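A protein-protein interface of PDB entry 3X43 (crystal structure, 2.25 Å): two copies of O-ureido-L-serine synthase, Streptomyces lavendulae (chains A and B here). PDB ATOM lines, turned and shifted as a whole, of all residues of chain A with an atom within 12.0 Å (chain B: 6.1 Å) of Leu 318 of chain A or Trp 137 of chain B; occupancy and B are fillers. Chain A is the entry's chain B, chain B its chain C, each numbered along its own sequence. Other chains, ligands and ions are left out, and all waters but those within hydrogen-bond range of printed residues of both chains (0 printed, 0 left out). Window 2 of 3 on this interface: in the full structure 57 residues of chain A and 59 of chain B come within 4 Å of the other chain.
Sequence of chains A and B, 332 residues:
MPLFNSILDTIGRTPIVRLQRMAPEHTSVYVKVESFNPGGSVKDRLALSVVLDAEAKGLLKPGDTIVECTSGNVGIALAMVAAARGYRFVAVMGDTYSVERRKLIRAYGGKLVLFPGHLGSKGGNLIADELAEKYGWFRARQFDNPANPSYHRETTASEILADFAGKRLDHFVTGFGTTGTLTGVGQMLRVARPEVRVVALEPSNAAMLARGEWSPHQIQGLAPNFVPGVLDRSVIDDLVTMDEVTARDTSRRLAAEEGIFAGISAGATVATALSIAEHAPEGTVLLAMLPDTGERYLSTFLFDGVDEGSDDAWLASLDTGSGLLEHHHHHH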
ATOM      1  N   SER A 310      13.429 -12.073  33.603  1.00  0.00           N
ATOM      2  CA  SER A 310      12.769 -11.137  32.700  1.00  0.00           C
ATOM      3  C   SER A 310      11.404 -11.660  32.255  1.00  0.00           C
ATOM      4  O   SER A 310      11.177 -12.870  32.195  1.00  0.00           O
ATOM      5  CB  SER A 310      13.655 -10.881  31.475  1.00  0.00           C
ATOM      6  OG  SER A 310      13.392  -9.612  30.895  1.00  0.00           O
ATOM      7  N   ASP A 311      10.503 -10.732  31.946  1.00  0.00           N
ATOM      8  CA  ASP A 311       9.148 -11.060  31.509  1.00  0.00           C
ATOM      9  C   ASP A 311       9.051 -11.251  29.994  1.00  0.00           C
ATOM     10  O   ASP A 311       8.156 -10.700  29.346  1.00  0.00           O
ATOM     11  CB  ASP A 311       8.186  -9.950  31.941  1.00  0.00           C
ATOM     12  CG  ASP A 311       7.459 -10.278  33.226  1.00  0.00           C
ATOM     13  OD1 ASP A 311       7.562 -11.438  33.680  1.00  0.00           O
ATOM     14  OD2 ASP A 311       6.786  -9.381  33.782  1.00  0.00           O
ATOM     15  N   ASP A 312       9.964 -12.042  29.440  1.00  0.00           N
ATOM     16  CA  ASP A 312       9.997 -12.305  28.002  1.00  0.00           C
ATOM     17  C   ASP A 312       8.654 -12.803  27.468  1.00  0.00           C
ATOM     18  O   ASP A 312       8.150 -12.309  26.456  1.00  0.00           O
ATOM     19  CB  ASP A 312      11.089 -13.332  27.686  1.00  0.00           C
ATOM     20  CG  ASP A 312      12.463 -12.890  28.170  1.00  0.00           C
ATOM     21  OD1 ASP A 312      13.039 -13.576  29.043  1.00  0.00           O
ATOM     22  OD2 ASP A 312      12.968 -11.853  27.679  1.00  0.00           O
ATOM     23  N   ALA A 313       8.077 -13.784  28.152  1.00  0.00           N
ATOM     24  CA  ALA A 313       6.803 -14.339  27.732  1.00  0.00           C
ATOM     25  C   ALA A 313       5.805 -13.216  27.523  1.00  0.00           C
ATOM     26  O   ALA A 313       5.172 -13.131  26.466  1.00  0.00           O
ATOM     27  CB  ALA A 313       6.284 -15.312  28.774  1.00  0.00           C
ATOM     28  N   TRP A 314       5.676 -12.349  28.529  1.00  0.00           N
ATOM     29  CA  TRP A 314       4.744 -11.228  28.456  1.00  0.00           C
ATOM     30  C   TRP A 314       5.040 -10.299  27.282  1.00  0.00           C
ATOM     31  O   TRP A 314       4.121  -9.847  26.602  1.00  0.00           O
ATOM     32  CB  TRP A 314       4.749 -10.419  29.760  1.00  0.00           C
ATOM     33  CG  TRP A 314       3.954  -9.141  29.635  1.00  0.00           C
ATOM     34  CD1 TRP A 314       2.602  -9.025  29.420  1.00  0.00           C
ATOM     35  CD2 TRP A 314       4.473  -7.804  29.631  1.00  0.00           C
ATOM     36  NE1 TRP A 314       2.254  -7.703  29.279  1.00  0.00           N
ATOM     37  CE2 TRP A 314       3.381  -6.931  29.404  1.00  0.00           C
ATOM     38  CE3 TRP A 314       5.754  -7.258  29.795  1.00  0.00           C
ATOM     39  CZ2 TRP A 314       3.533  -5.544  29.337  1.00  0.00           C
ATOM     40  CZ3 TRP A 314       5.904  -5.872  29.727  1.00  0.00           C
ATOM     41  CH2 TRP A 314       4.798  -5.037  29.500  1.00  0.00           C
ATOM     42  N   LEU A 315       6.313 -10.005  27.045  1.00  0.00           N
ATOM     43  CA  LEU A 315       6.673  -9.133  25.926  1.00  0.00           C
ATOM     44  C   LEU A 315       6.239  -9.794  24.616  1.00  0.00           C
ATOM     45  O   LEU A 315       5.731  -9.132  23.705  1.00  0.00           O
ATOM     46  CB  LEU A 315       8.186  -8.885  25.895  1.00  0.00           C
ATOM     47  CG  LEU A 315       8.802  -7.905  26.902  1.00  0.00           C
ATOM     48  CD1 LEU A 315      10.308  -7.906  26.738  1.00  0.00           C
ATOM     49  CD2 LEU A 315       8.244  -6.501  26.689  1.00  0.00           C
ATOM     50  N   ALA A 316       6.441 -11.109  24.540  1.00  0.00           N
ATOM     51  CA  ALA A 316       6.088 -11.883  23.357  1.00  0.00           C
ATOM     52  C   ALA A 316       4.592 -11.806  23.054  1.00  0.00           C
ATOM     53  O   ALA A 316       4.197 -11.668  21.896  1.00  0.00           O
ATOM     54  CB  ALA A 316       6.520 -13.338  23.537  1.00  0.00           C
ATOM     55  N   SER A 317       3.769 -11.889  24.093  1.00  0.00           N
ATOM     56  CA  SER A 317       2.317 -11.827  23.931  1.00  0.00           C
ATOM     57  C   SER A 317       1.835 -10.462  23.442  1.00  0.00           C
ATOM     58  O   SER A 317       0.662 -10.293  23.110  1.00  0.00           O
ATOM     59  CB  SER A 317       1.621 -12.164  25.259  1.00  0.00           C
ATOM     60  OG  SER A 317       1.436 -11.007  26.062  1.00  0.00           O
ATOM     61  N   LEU A 318       2.738  -9.490  23.402  1.00  0.00           N
ATOM     62  CA  LEU A 318       2.381  -8.143  22.966  1.00  0.00           C
ATOM     63  C   LEU A 318       2.448  -7.961  21.454  1.00  0.00           C
ATOM     64  O   LEU A 318       1.686  -7.177  20.886  1.00  0.00           O
ATOM     65  CB  LEU A 318       3.290  -7.111  23.640  1.00  0.00           C
ATOM     66  CG  LEU A 318       3.137  -6.964  25.155  1.00  0.00           C
ATOM     67  CD1 LEU A 318       4.295  -6.139  25.698  1.00  0.00           C
ATOM     68  CD2 LEU A 318       1.793  -6.318  25.487  1.00  0.00           C
ATOM     69  N   ASP A 319       3.354  -8.684  20.803  1.00  0.00           N
ATOM     70  CA  ASP A 319       3.506  -8.578  19.354  1.00  0.00           C
ATOM     71  C   ASP A 319       2.870  -9.739  18.585  1.00  0.00           C
ATOM     72  O   ASP A 319       3.206  -9.974  17.420  1.00  0.00           O
ATOM     73  CB  ASP A 319       4.993  -8.469  18.992  1.00  0.00           C
ATOM     74  CG  ASP A 319       5.444  -7.028  18.791  1.00  0.00           C
ATOM     75  OD1 ASP A 319       4.585  -6.119  18.860  1.00  0.00           O
ATOM     76  OD2 ASP A 319       6.656  -6.802  18.563  1.00  0.00           O
ATOM     77  N   THR A 320       1.955 -10.457  19.233  1.00  0.00           N
ATOM     78  CA  THR A 320       1.275 -11.591  18.601  1.00  0.00           C
ATOM     79  C   THR A 320      -0.145 -11.783  19.134  1.00  0.00           C
ATOM     80  O   THR A 320      -0.340 -11.643  20.359  1.00  0.00           O
ATOM     81  CB  THR A 320       2.052 -12.921  18.814  1.00  0.00           C
ATOM     82  OG1 THR A 320       2.503 -13.005  20.173  1.00  0.00           O
ATOM     83  CG2 THR A 320       3.249 -13.006  17.868  1.00  0.00           C
ATOM     84  N   THR B  65       0.071   2.189  30.325  1.00  0.00           N
ATOM     85  CA  THR B  65       1.220   1.583  30.979  1.00  0.00           C
ATOM     86  C   THR B  65       2.370   2.586  31.030  1.00  0.00           C
ATOM     87  O   THR B  65       2.514   3.440  30.154  1.00  0.00           O
ATOM     88  CB  THR B  65       1.659   0.254  30.282  1.00  0.00           C
ATOM     89  OG1 THR B  65       2.960   0.409  29.704  1.00  0.00           O
ATOM     90  CG2 THR B  65       0.645  -0.157  29.223  1.00  0.00           C
ATOM     91  N   ILE B  66       3.157   2.491  32.093  1.00  0.00           N
ATOM     92  CA  ILE B  66       4.285   3.378  32.331  1.00  0.00           C
ATOM     93  C   ILE B  66       5.580   2.576  32.283  1.00  0.00           C
ATOM     94  O   ILE B  66       5.651   1.488  32.842  1.00  0.00           O
ATOM     95  CB  ILE B  66       4.162   4.041  33.744  1.00  0.00           C
ATOM     96  CG1 ILE B  66       2.936   4.965  33.784  1.00  0.00           C
ATOM     97  CG2 ILE B  66       5.444   4.785  34.098  1.00  0.00           C
ATOM     98  CD1 ILE B  66       2.299   5.132  35.178  1.00  0.00           C
ATOM     99  N   VAL B  67       6.593   3.114  31.607  1.00  0.00           N
ATOM    100  CA  VAL B  67       7.892   2.450  31.517  1.00  0.00           C
ATOM    101  C   VAL B  67       8.964   3.373  32.033  1.00  0.00           C
ATOM    102  O   VAL B  67       8.914   4.576  31.787  1.00  0.00           O
ATOM    103  CB  VAL B  67       8.318   2.111  30.075  1.00  0.00           C
ATOM    104  CG1 VAL B  67       8.384   0.615  29.904  1.00  0.00           C
ATOM    105  CG2 VAL B  67       7.387   2.770  29.073  1.00  0.00           C
ATOM    106  N   ARG B  88      -0.445   0.057  34.256  1.00  0.00           N
ATOM    107  CA  ARG B  88       0.482  -1.044  34.129  1.00  0.00           C
ATOM    108  C   ARG B  88       1.845  -0.380  34.215  1.00  0.00           C
ATOM    109  O   ARG B  88       2.039   0.702  33.669  1.00  0.00           O
ATOM    110  CB  ARG B  88       0.312  -1.714  32.770  1.00  0.00           C
ATOM    111  CG  ARG B  88       0.406  -3.227  32.803  1.00  0.00           C
ATOM    112  CD  ARG B  88       1.082  -3.747  31.550  1.00  0.00           C
ATOM    113  NE  ARG B  88       0.179  -4.527  30.703  1.00  0.00           N
ATOM    114  CZ  ARG B  88       0.016  -4.326  29.395  1.00  0.00           C
ATOM    115  NH1 ARG B  88       0.690  -3.363  28.769  1.00  0.00           N
ATOM    116  NH2 ARG B  88      -0.806  -5.107  28.705  1.00  0.00           N
ATOM    117  N   VAL B  90       6.166  -0.925  33.815  1.00  0.00           N
ATOM    118  CA  VAL B  90       7.243  -1.771  33.306  1.00  0.00           C
ATOM    119  C   VAL B  90       8.614  -1.249  33.728  1.00  0.00           C
ATOM    120  O   VAL B  90       9.032  -0.159  33.328  1.00  0.00           O
ATOM    121  CB  VAL B  90       7.228  -1.855  31.770  1.00  0.00           C
ATOM    122  CG1 VAL B  90       8.463  -2.611  31.288  1.00  0.00           C
ATOM    123  CG2 VAL B  90       5.953  -2.535  31.295  1.00  0.00           C
ATOM    124  N   ALA B 128      14.282   1.400  27.351  1.00  0.00           N
ATOM    125  CA  ALA B 128      13.025   1.988  27.797  1.00  0.00           C
ATOM    126  C   ALA B 128      12.472   2.906  26.729  1.00  0.00           C
ATOM    127  O   ALA B 128      11.281   2.867  26.427  1.00  0.00           O
ATOM    128  CB  ALA B 128      13.237   2.765  29.090  1.00  0.00           C
ATOM    129  N   LEU B 131      11.060   0.627  23.864  1.00  0.00           N
ATOM    130  CA  LEU B 131       9.770   0.033  24.202  1.00  0.00           C
ATOM    131  C   LEU B 131       8.674   1.086  24.156  1.00  0.00           C
ATOM    132  O   LEU B 131       7.615   0.880  23.552  1.00  0.00           O
ATOM    133  CB  LEU B 131       9.812  -0.571  25.603  1.00  0.00           C
ATOM    134  CG  LEU B 131      10.727  -1.776  25.801  1.00  0.00           C
ATOM    135  CD1 LEU B 131      10.805  -2.101  27.276  1.00  0.00           C
ATOM    136  CD2 LEU B 131      10.198  -2.970  25.021  1.00  0.00           C
ATOM    137  N   ALA B 132       8.947   2.213  24.807  1.00  0.00           N
ATOM    138  CA  ALA B 132       8.016   3.325  24.884  1.00  0.00           C
ATOM    139  C   ALA B 132       7.470   3.726  23.522  1.00  0.00           C
ATOM    140  O   ALA B 132       6.264   3.925  23.368  1.00  0.00           O
ATOM    141  CB  ALA B 132       8.694   4.512  25.544  1.00  0.00           C
ATOM    142  N   GLU B 133       8.358   3.848  22.536  1.00  0.00           N
ATOM    143  CA  GLU B 133       7.945   4.229  21.185  1.00  0.00           C
ATOM    144  C   GLU B 133       7.238   3.079  20.476  1.00  0.00           C
ATOM    145  O   GLU B 133       6.170   3.257  19.878  1.00  0.00           O
ATOM    146  CB  GLU B 133       9.149   4.675  20.346  1.00  0.00           C
ATOM    147  CG  GLU B 133      10.508   4.292  20.908  1.00  0.00           C
ATOM    148  CD  GLU B 133      11.623   5.242  20.467  1.00  0.00           C
ATOM    149  OE1 GLU B 133      11.352   6.455  20.304  1.00  0.00           O
ATOM    150  OE2 GLU B 133      12.771   4.778  20.283  1.00  0.00           O
ATOM    151  N   LYS B 134       7.842   1.898  20.560  1.00  0.00           N
ATOM    152  CA  LYS B 134       7.297   0.704  19.934  1.00  0.00           C
ATOM    153  C   LYS B 134       5.848   0.406  20.330  1.00  0.00           C
ATOM    154  O   LYS B 134       5.044   0.018  19.482  1.00  0.00           O
ATOM    155  CB  LYS B 134       8.184  -0.500  20.271  1.00  0.00           C
ATOM    156  CG  LYS B 134       7.705  -1.821  19.682  1.00  0.00           C
ATOM    157  CD  LYS B 134       8.871  -2.767  19.438  1.00  0.00           C
ATOM    158  CE  LYS B 134       8.564  -4.173  19.934  1.00  0.00           C
ATOM    159  NZ  LYS B 134       9.794  -4.876  20.419  1.00  0.00           N
ATOM    160  N   TYR B 135       5.509   0.598  21.604  1.00  0.00           N
ATOM    161  CA  TYR B 135       4.153   0.308  22.068  1.00  0.00           C
ATOM    162  C   TYR B 135       3.314   1.501  22.511  1.00  0.00           C
ATOM    163  O   TYR B 135       2.173   1.325  22.936  1.00  0.00           O
ATOM    164  CB  TYR B 135       4.194  -0.712  23.208  1.00  0.00           C
ATOM    165  CG  TYR B 135       4.927  -1.995  22.882  1.00  0.00           C
ATOM    166  CD1 TYR B 135       4.325  -2.991  22.110  1.00  0.00           C
ATOM    167  CD2 TYR B 135       6.212  -2.228  23.377  1.00  0.00           C
ATOM    168  CE1 TYR B 135       4.990  -4.195  21.845  1.00  0.00           C
ATOM    169  CE2 TYR B 135       6.879  -3.426  23.116  1.00  0.00           C
ATOM    170  CZ  TYR B 135       6.264  -4.404  22.353  1.00  0.00           C
ATOM    171  OH  TYR B 135       6.921  -5.594  22.114  1.00  0.00           O
ATOM    172  N   GLY B 136       3.870   2.705  22.424  1.00  0.00           N
ATOM    173  CA  GLY B 136       3.124   3.895  22.820  1.00  0.00           C
ATOM    174  C   GLY B 136       2.918   4.071  24.317  1.00  0.00           C
ATOM    175  O   GLY B 136       1.902   4.619  24.761  1.00  0.00           O
ATOM    176  N   TRP B 137       3.888   3.611  25.098  1.00  0.00           N
ATOM    177  CA  TRP B 137       3.811   3.719  26.547  1.00  0.00           C
ATOM    178  C   TRP B 137       4.322   5.086  27.004  1.00  0.00           C
ATOM    179  O   TRP B 137       4.983   5.804  26.243  1.00  0.00           O
ATOM    180  CB  TRP B 137       4.648   2.619  27.204  1.00  0.00           C
ATOM    181  CG  TRP B 137       4.191   1.198  26.926  1.00  0.00           C
ATOM    182  CD1 TRP B 137       2.943   0.787  26.536  1.00  0.00           C
ATOM    183  CD2 TRP B 137       4.976   0.005  27.070  1.00  0.00           C
ATOM    184  NE1 TRP B 137       2.906  -0.585  26.434  1.00  0.00           N
ATOM    185  CE2 TRP B 137       4.140  -1.088  26.756  1.00  0.00           C
ATOM    186  CE3 TRP B 137       6.307  -0.244  27.436  1.00  0.00           C
ATOM    187  CZ2 TRP B 137       4.593  -2.412  26.797  1.00  0.00           C
ATOM    188  CZ3 TRP B 137       6.757  -1.562  27.476  1.00  0.00           C
ATOM    189  CH2 TRP B 137       5.900  -2.627  27.158  1.00  0.00           C
ATOM    190  N   PHE B 138       4.011   5.434  28.253  1.00  0.00           N
ATOM    191  CA  PHE B 138       4.427   6.700  28.841  1.00  0.00           C
ATOM    192  C   PHE B 138       5.768   6.546  29.555  1.00  0.00           C
ATOM    193  O   PHE B 138       5.971   5.600  30.304  1.00  0.00           O
ATOM    194  CB  PHE B 138       3.364   7.189  29.835  1.00  0.00           C
ATOM    195  CG  PHE B 138       3.819   8.332  30.704  1.00  0.00           C
ATOM    196  CD1 PHE B 138       3.649   9.652  30.288  1.00  0.00           C
ATOM    197  CD2 PHE B 138       4.413   8.090  31.944  1.00  0.00           C
ATOM    198  CE1 PHE B 138       4.064  10.717  31.093  1.00  0.00           C
ATOM    199  CE2 PHE B 138       4.836   9.147  32.759  1.00  0.00           C
ATOM    200  CZ  PHE B 138       4.659  10.466  32.330  1.00  0.00           C
ATOM    201  N   ARG B 139       6.676   7.483  29.318  1.00  0.00           N
ATOM    202  CA  ARG B 139       7.998   7.461  29.942  1.00  0.00           C
ATOM    203  C   ARG B 139       8.051   8.505  31.069  1.00  0.00           C
ATOM    204  O   ARG B 139       7.773   9.677  30.840  1.00  0.00           O
ATOM    205  CB  ARG B 139       9.072   7.777  28.893  1.00  0.00           C
ATOM    206  CG  ARG B 139       9.548   6.575  28.097  1.00  0.00           C
ATOM    207  CD  ARG B 139      11.064   6.420  28.192  1.00  0.00           C
ATOM    208  NE  ARG B 139      11.506   6.287  29.576  1.00  0.00           N
ATOM    209  CZ  ARG B 139      12.774   6.345  29.968  1.00  0.00           C
ATOM    210  NH1 ARG B 139      13.740   6.536  29.077  1.00  0.00           N
ATOM    211  NH2 ARG B 139      13.078   6.212  31.254  1.00  0.00           N
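The backbone carbonyl oxygen (O) of Trp 314 of chain A sits at hydrogen-bond distance from the side-chain hydroxyl (OG) of Ser 317 of chain A (3.0 Å).
The side-chain hydroxyl of Thr 65 of chain B lies close to the indole nitrogen of Trp 137 of chain B, at 3.4 Å.
The backbone NH of Ile 66 of chain B is in hydrogen-bond range of the backbone carbonyl oxygen of Arg 88 of chain B, at 2.6 Å.
The backbone carbonyl oxygen (O) of Ile 66 of chain B is in hydrogen-bond range of the backbone NH (N) of Val 90 of chain B (2.7 Å).
The backbone NH (N) of Trp 137 of chain B sits at hydrogen-bond distance from the backbone carbonyl oxygen (O) of Ala 132 of chain B, 3.0 Å away.
The side-chain amino group of Lys 134 of chain B lies close to the side-chain hydroxyl of Tyr 135 of chain B (3.4 Å).
Trp 314 of chain A touches Arg 88 of chain B.
Val 90 of chain B touches Trp 314 of chain A (CG2 to CH2, 3.3 Å).
Trp 137 of chain B touches Trp 314 of chain A.
Leu 318 of chain A touches Tyr 135 of chain B (CB to CE1, 3.8 Å).
CZ2 of Trp 137 of chain B touches CD1 of Leu 318 of chain A, at 3.9 Å.
CE of Lys 134 of chain B touches OD2 of Asp 319 of chain A (3.5 Å).
Tyr 135 of chain B touches Asp 319 of chain A.
Of chain B, only Tyr 135 and Trp 137 come within 4 Å of Leu 318 of chain A.
Of the printed residues of chain B, Asp 319 of chain A touches Lys 134 (3.5 Å) and Tyr 135 (3.6 Å).
No residue of chain A comes within 4 Å of Thr 65 of chain B.
No residue of chain A comes within 4 Å of Val 67 of chain B.
Of chain A, only Trp 314 comes within 4 Å of Val 90 of chain B.
Ala 128 of chain B touches none of the printed residues of chain A.
Leu 131 of chain B touches none of the printed residues of chain A.
Of the printed residues of chain A, Lys 134 of chain B touches Asp 319 (3.5 Å).
Tyr 135 of chain B touches two residues of chain A.
No residue of chain A comes within 4 Å of Gly 136 of chain B.
Trp 137 of chain B touches two residues of chain A.
No residue of chain A comes within 4 Å of Phe 138 of chain B.
The nearest residue of chain A that does not touch Trp 137 of chain B is Leu 315 of chain A (4.6 Å).
The nearest printed residue of chain A that does not touch Arg 88 of chain B is Leu 318 of chain A (4.3 Å).
Hydrophobic or aromatic side chains of chain A that line the printed part of chain B: Trp 314 and Leu 318.
Of the 15 printed residues of chain B, 5 touch a printed residue of chain A.
No position is printed for both chains.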
